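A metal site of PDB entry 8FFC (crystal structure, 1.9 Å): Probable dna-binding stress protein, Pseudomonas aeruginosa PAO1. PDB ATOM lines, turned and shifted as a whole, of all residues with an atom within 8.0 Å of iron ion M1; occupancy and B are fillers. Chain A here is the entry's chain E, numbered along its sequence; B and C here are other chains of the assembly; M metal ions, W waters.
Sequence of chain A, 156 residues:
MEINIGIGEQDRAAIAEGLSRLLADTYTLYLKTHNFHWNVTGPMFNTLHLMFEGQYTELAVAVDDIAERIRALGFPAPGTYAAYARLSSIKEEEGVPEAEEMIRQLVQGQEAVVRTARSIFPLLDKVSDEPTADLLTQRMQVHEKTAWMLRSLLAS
His 49 of chain B touches iron ion M1 (CE1 to FE, 3.99 Å).
Iron ion M1 is bound by the side-chain carboxylate (OE2) of Glu 68 (2.2 Å), a ring nitrogen (NE2) of His 37 of chain B (2.2 Å), the side-chain carboxylate (OD2) of Asp 64 (2.3 Å), water W1 (2.3 Å) and the side-chain carboxylate (OD1) of Asp 64 (2.4 Å).
The side-chain carboxylate of Glu 68 lies within salt-bridge range of the side-chain amino group of Lys 145 of chain C (3.4 Å).
ND1 of His 37 of chain B sits at hydrogen-bond distance from O of His 49 of chain B (2.7 Å).
The side-chain carboxylate of Asp 64 lies close to the indole nitrogen of Trp 38 of chain B (2.9 Å).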
ATOM      1  N   ALA A  60      14.633  31.226 -15.962  1.00  0.00           N
ATOM      2  CA  ALA A  60      14.051  31.787 -17.176  1.00  0.00           C
ATOM      3  C   ALA A  60      13.598  30.678 -18.117  1.00  0.00           C
ATOM      4  O   ALA A  60      12.558  30.801 -18.793  1.00  0.00           O
ATOM      5  CB  ALA A  60      15.059  32.688 -17.876  1.00  0.00           C
ATOM      6  N   VAL A  61      14.351  29.583 -18.176  1.00  0.00           N
ATOM      7  CA  VAL A  61      13.924  28.414 -18.927  1.00  0.00           C
ATOM      8  C   VAL A  61      12.694  27.779 -18.280  1.00  0.00           C
ATOM      9  O   VAL A  61      11.782  27.303 -18.981  1.00  0.00           O
ATOM     10  CB  VAL A  61      15.092  27.408 -19.020  1.00  0.00           C
ATOM     11  CG1 VAL A  61      14.609  26.103 -19.649  1.00  0.00           C
ATOM     12  CG2 VAL A  61      16.311  28.021 -19.779  1.00  0.00           C
ATOM     13  N   VAL A  63      10.305  29.146 -16.529  1.00  0.00           N
ATOM     14  CA  VAL A  63       9.135  29.976 -16.834  1.00  0.00           C
ATOM     15  C   VAL A  63       8.600  29.615 -18.211  1.00  0.00           C
ATOM     16  O   VAL A  63       7.387  29.504 -18.445  1.00  0.00           O
ATOM     17  CB  VAL A  63       9.528  31.462 -16.724  1.00  0.00           C
ATOM     18  CG1 VAL A  63       8.685  32.362 -17.579  1.00  0.00           C
ATOM     19  CG2 VAL A  63       9.457  31.936 -15.277  1.00  0.00           C
ATOM     20  N   ASP A  64       9.507  29.464 -19.178  1.00  0.00           N
ATOM     21  CA  ASP A  64       9.071  29.124 -20.529  1.00  0.00           C
ATOM     22  C   ASP A  64       8.432  27.737 -20.558  1.00  0.00           C
ATOM     23  O   ASP A  64       7.402  27.543 -21.206  1.00  0.00           O
ATOM     24  CB  ASP A  64      10.249  29.249 -21.500  1.00  0.00           C
ATOM     25  CG  ASP A  64       9.813  29.176 -22.950  1.00  0.00           C
ATOM     26  OD1 ASP A  64       9.206  30.153 -23.439  1.00  0.00           O
ATOM     27  OD2 ASP A  64      10.052  28.127 -23.569  1.00  0.00           O
ATOM     28  N   ASP A  65       9.011  26.767 -19.861  1.00  0.00           N
ATOM     29  CA  ASP A  65       8.455  25.418 -19.874  1.00  0.00           C
ATOM     30  C   ASP A  65       7.098  25.349 -19.172  1.00  0.00           C
ATOM     31  O   ASP A  65       6.198  24.604 -19.603  1.00  0.00           O
ATOM     32  CB  ASP A  65       9.425  24.459 -19.195  1.00  0.00           C
ATOM     33  CG  ASP A  65      10.630  24.132 -20.061  1.00  0.00           C
ATOM     34  OD1 ASP A  65      10.601  24.374 -21.276  1.00  0.00           O
ATOM     35  OD2 ASP A  65      11.598  23.608 -19.495  1.00  0.00           O
ATOM     36  N   ALA A  67       4.932  27.887 -18.817  1.00  0.00           N
ATOM     37  CA  ALA A  67       3.984  28.609 -19.675  1.00  0.00           C
ATOM     38  C   ALA A  67       3.572  27.773 -20.873  1.00  0.00           C
ATOM     39  O   ALA A  67       2.399  27.773 -21.261  1.00  0.00           O
ATOM     40  CB  ALA A  67       4.597  29.937 -20.140  1.00  0.00           C
ATOM     41  N   GLU A  68       4.507  27.063 -21.499  1.00  0.00           N
ATOM     42  CA  GLU A  68       4.117  26.272 -22.664  1.00  0.00           C
ATOM     43  C   GLU A  68       3.365  24.990 -22.295  1.00  0.00           C
ATOM     44  O   GLU A  68       2.604  24.477 -23.130  1.00  0.00           O
ATOM     45  CB  GLU A  68       5.353  25.977 -23.537  1.00  0.00           C
ATOM     46  CG  GLU A  68       5.933  27.256 -24.067  1.00  0.00           C
ATOM     47  CD  GLU A  68       7.138  27.090 -25.007  1.00  0.00           C
ATOM     48  OE1 GLU A  68       7.750  26.007 -25.094  1.00  0.00           O
ATOM     49  OE2 GLU A  68       7.423  28.096 -25.654  1.00  0.00           O
ATOM     50  N   HIS B  34       7.874  38.082 -24.242  1.00  0.00           N
ATOM     51  CA  HIS B  34       7.809  36.698 -23.787  1.00  0.00           C
ATOM     52  C   HIS B  34       6.357  36.205 -23.769  1.00  0.00           C
ATOM     53  O   HIS B  34       6.070  35.069 -24.159  1.00  0.00           O
ATOM     54  CB  HIS B  34       8.418  36.609 -22.383  1.00  0.00           C
ATOM     55  CG  HIS B  34       9.135  35.339 -22.090  1.00  0.00           C
ATOM     56  ND1 HIS B  34       8.852  34.142 -22.734  1.00  0.00           N
ATOM     57  CD2 HIS B  34      10.133  35.071 -21.222  1.00  0.00           C
ATOM     58  CE1 HIS B  34       9.649  33.204 -22.264  1.00  0.00           C
ATOM     59  NE2 HIS B  34      10.433  33.737 -21.346  1.00  0.00           N
ATOM     60  N   HIS B  37       5.258  35.552 -27.264  1.00  0.00           N
ATOM     61  CA  HIS B  37       5.880  34.308 -27.708  1.00  0.00           C
ATOM     62  C   HIS B  37       5.034  33.096 -27.331  1.00  0.00           C
ATOM     63  O   HIS B  37       4.890  32.169 -28.127  1.00  0.00           O
ATOM     64  CB  HIS B  37       7.310  34.221 -27.119  1.00  0.00           C
ATOM     65  CG  HIS B  37       7.929  32.859 -27.106  1.00  0.00           C
ATOM     66  ND1 HIS B  37       8.591  32.318 -28.201  1.00  0.00           N
ATOM     67  CD2 HIS B  37       8.091  31.973 -26.098  1.00  0.00           C
ATOM     68  CE1 HIS B  37       9.063  31.139 -27.879  1.00  0.00           C
ATOM     69  NE2 HIS B  37       8.778  30.902 -26.611  1.00  0.00           N
ATOM     70  N   TRP B  38       4.457  33.094 -26.121  1.00  0.00           N
ATOM     71  CA  TRP B  38       3.676  31.932 -25.689  1.00  0.00           C
ATOM     72  C   TRP B  38       2.319  31.899 -26.369  1.00  0.00           C
ATOM     73  O   TRP B  38       1.793  30.817 -26.671  1.00  0.00           O
ATOM     74  CB  TRP B  38       3.441  31.971 -24.187  1.00  0.00           C
ATOM     75  CG  TRP B  38       4.661  31.912 -23.379  1.00  0.00           C
ATOM     76  CD1 TRP B  38       5.778  31.170 -23.624  1.00  0.00           C
ATOM     77  CD2 TRP B  38       4.912  32.628 -22.174  1.00  0.00           C
ATOM     78  NE1 TRP B  38       6.722  31.371 -22.641  1.00  0.00           N
ATOM     79  CE2 TRP B  38       6.217  32.273 -21.733  1.00  0.00           C
ATOM     80  CE3 TRP B  38       4.159  33.516 -21.401  1.00  0.00           C
ATOM     81  CZ2 TRP B  38       6.775  32.785 -20.569  1.00  0.00           C
ATOM     82  CZ3 TRP B  38       4.723  34.049 -20.246  1.00  0.00           C
ATOM     83  CH2 TRP B  38       6.021  33.666 -19.836  1.00  0.00           C
ATOM     84  N   HIS B  49       6.622  32.892 -33.042  1.00  0.00           N
ATOM     85  CA  HIS B  49       7.137  32.206 -31.857  1.00  0.00           C
ATOM     86  C   HIS B  49       8.664  32.289 -31.837  1.00  0.00           C
ATOM     87  O   HIS B  49       9.275  32.638 -30.817  1.00  0.00           O
ATOM     88  CB  HIS B  49       6.649  30.765 -31.890  1.00  0.00           C
ATOM     89  CG  HIS B  49       6.950  29.961 -30.651  1.00  0.00           C
ATOM     90  ND1 HIS B  49       6.361  30.202 -29.432  1.00  0.00           N
ATOM     91  CD2 HIS B  49       7.735  28.865 -30.478  1.00  0.00           C
ATOM     92  CE1 HIS B  49       6.777  29.311 -28.551  1.00  0.00           C
ATOM     93  NE2 HIS B  49       7.617  28.493 -29.166  1.00  0.00           N
ATOM     94  N   GLU B  53      11.107  34.794 -29.527  1.00  0.00           N
ATOM     95  CA  GLU B  53      12.117  34.138 -28.693  1.00  0.00           C
ATOM     96  C   GLU B  53      13.460  34.846 -28.810  1.00  0.00           C
ATOM     97  O   GLU B  53      14.120  35.150 -27.808  1.00  0.00           O
ATOM     98  CB  GLU B  53      12.230  32.665 -29.064  1.00  0.00           C
ATOM     99  CG  GLU B  53      13.219  31.901 -28.235  1.00  0.00           C
ATOM    100  CD  GLU B  53      13.190  30.413 -28.555  1.00  0.00           C
ATOM    101  OE1 GLU B  53      13.575  30.060 -29.689  1.00  0.00           O
ATOM    102  OE2 GLU B  53      12.796  29.604 -27.686  1.00  0.00           O
ATOM    103  N   TYR B  56      13.234  38.357 -26.923  1.00  0.00           N
ATOM    104  CA  TYR B  56      13.265  38.403 -25.466  1.00  0.00           C
ATOM    105  C   TYR B  56      14.577  37.874 -24.931  1.00  0.00           C
ATOM    106  O   TYR B  56      15.043  38.305 -23.876  1.00  0.00           O
ATOM    107  CB  TYR B  56      12.088  37.661 -24.850  1.00  0.00           C
ATOM    108  CG  TYR B  56      12.097  36.151 -24.778  1.00  0.00           C
ATOM    109  CD1 TYR B  56      12.966  35.475 -23.952  1.00  0.00           C
ATOM    110  CD2 TYR B  56      11.144  35.403 -25.442  1.00  0.00           C
ATOM    111  CE1 TYR B  56      12.966  34.114 -23.874  1.00  0.00           C
ATOM    112  CE2 TYR B  56      11.142  34.033 -25.374  1.00  0.00           C
ATOM    113  CZ  TYR B  56      12.046  33.400 -24.576  1.00  0.00           C
ATOM    114  OH  TYR B  56      12.073  32.029 -24.456  1.00  0.00           O
ATOM    115  N   LYS C 145       2.869  18.712 -26.554  1.00  0.00           N
ATOM    116  CA  LYS C 145       3.436  20.006 -26.923  1.00  0.00           C
ATOM    117  C   LYS C 145       3.399  20.215 -28.431  1.00  0.00           C
ATOM    118  O   LYS C 145       3.114  21.327 -28.916  1.00  0.00           O
ATOM    119  CB  LYS C 145       4.877  20.119 -26.436  1.00  0.00           C
ATOM    120  CG  LYS C 145       5.521  21.415 -26.861  1.00  0.00           C
ATOM    121  CD  LYS C 145       6.993  21.489 -26.383  1.00  0.00           C
ATOM    122  CE  LYS C 145       7.672  22.804 -26.785  1.00  0.00           C
ATOM    123  NZ  LYS C 145       8.970  22.999 -26.063  1.00  0.00           N
ATOM    124  N   TRP C 148       0.049  21.258 -29.694  1.00  0.00           N
ATOM    125  CA  TRP C 148      -0.226  22.684 -29.494  1.00  0.00           C
ATOM    126  C   TRP C 148       0.429  23.533 -30.577  1.00  0.00           C
ATOM    127  O   TRP C 148      -0.193  24.447 -31.159  1.00  0.00           O
ATOM    128  CB  TRP C 148       0.231  23.140 -28.087  1.00  0.00           C
ATOM    129  CG  TRP C 148       0.688  24.581 -28.066  1.00  0.00           C
ATOM    130  CD1 TRP C 148      -0.070  25.684 -28.317  1.00  0.00           C
ATOM    131  CD2 TRP C 148       2.008  25.065 -27.782  1.00  0.00           C
ATOM    132  NE1 TRP C 148       0.688  26.813 -28.231  1.00  0.00           N
ATOM    133  CE2 TRP C 148       1.970  26.470 -27.881  1.00  0.00           C
ATOM    134  CE3 TRP C 148       3.217  24.440 -27.437  1.00  0.00           C
ATOM    135  CZ2 TRP C 148       3.106  27.273 -27.675  1.00  0.00           C
ATOM    136  CZ3 TRP C 148       4.347  25.256 -27.231  1.00  0.00           C
ATOM    137  CH2 TRP C 148       4.282  26.638 -27.352  1.00  0.00           C
ATOM    138  N   MET C 149       1.693  23.242 -30.897  1.00  0.00           N
ATOM    139  CA  MET C 149       2.391  24.032 -31.900  1.00  0.00           C
ATOM    140  C   MET C 149       1.731  23.884 -33.276  1.00  0.00           C
ATOM    141  O   MET C 149       1.545  24.875 -33.990  1.00  0.00           O
ATOM    142  CB  MET C 149       3.856  23.614 -31.943  1.00  0.00           C
ATOM    143  CG  MET C 149       4.555  23.961 -30.607  1.00  0.00           C
ATOM    144  SD  MET C 149       6.299  23.599 -30.672  1.00  0.00           S
ATOM    145  CE  MET C 149       6.700  25.105 -31.533  1.00  0.00           C
HETATM  146 FE    FE M   1       9.384  29.058 -25.535  1.00  0.00          FE
HETATM  147 FE    FE M   2       9.339  27.414 -27.466  1.00  0.00          FE
HETATM  148  O   HOH W   1      11.596  29.813 -25.651  1.00  0.00           O
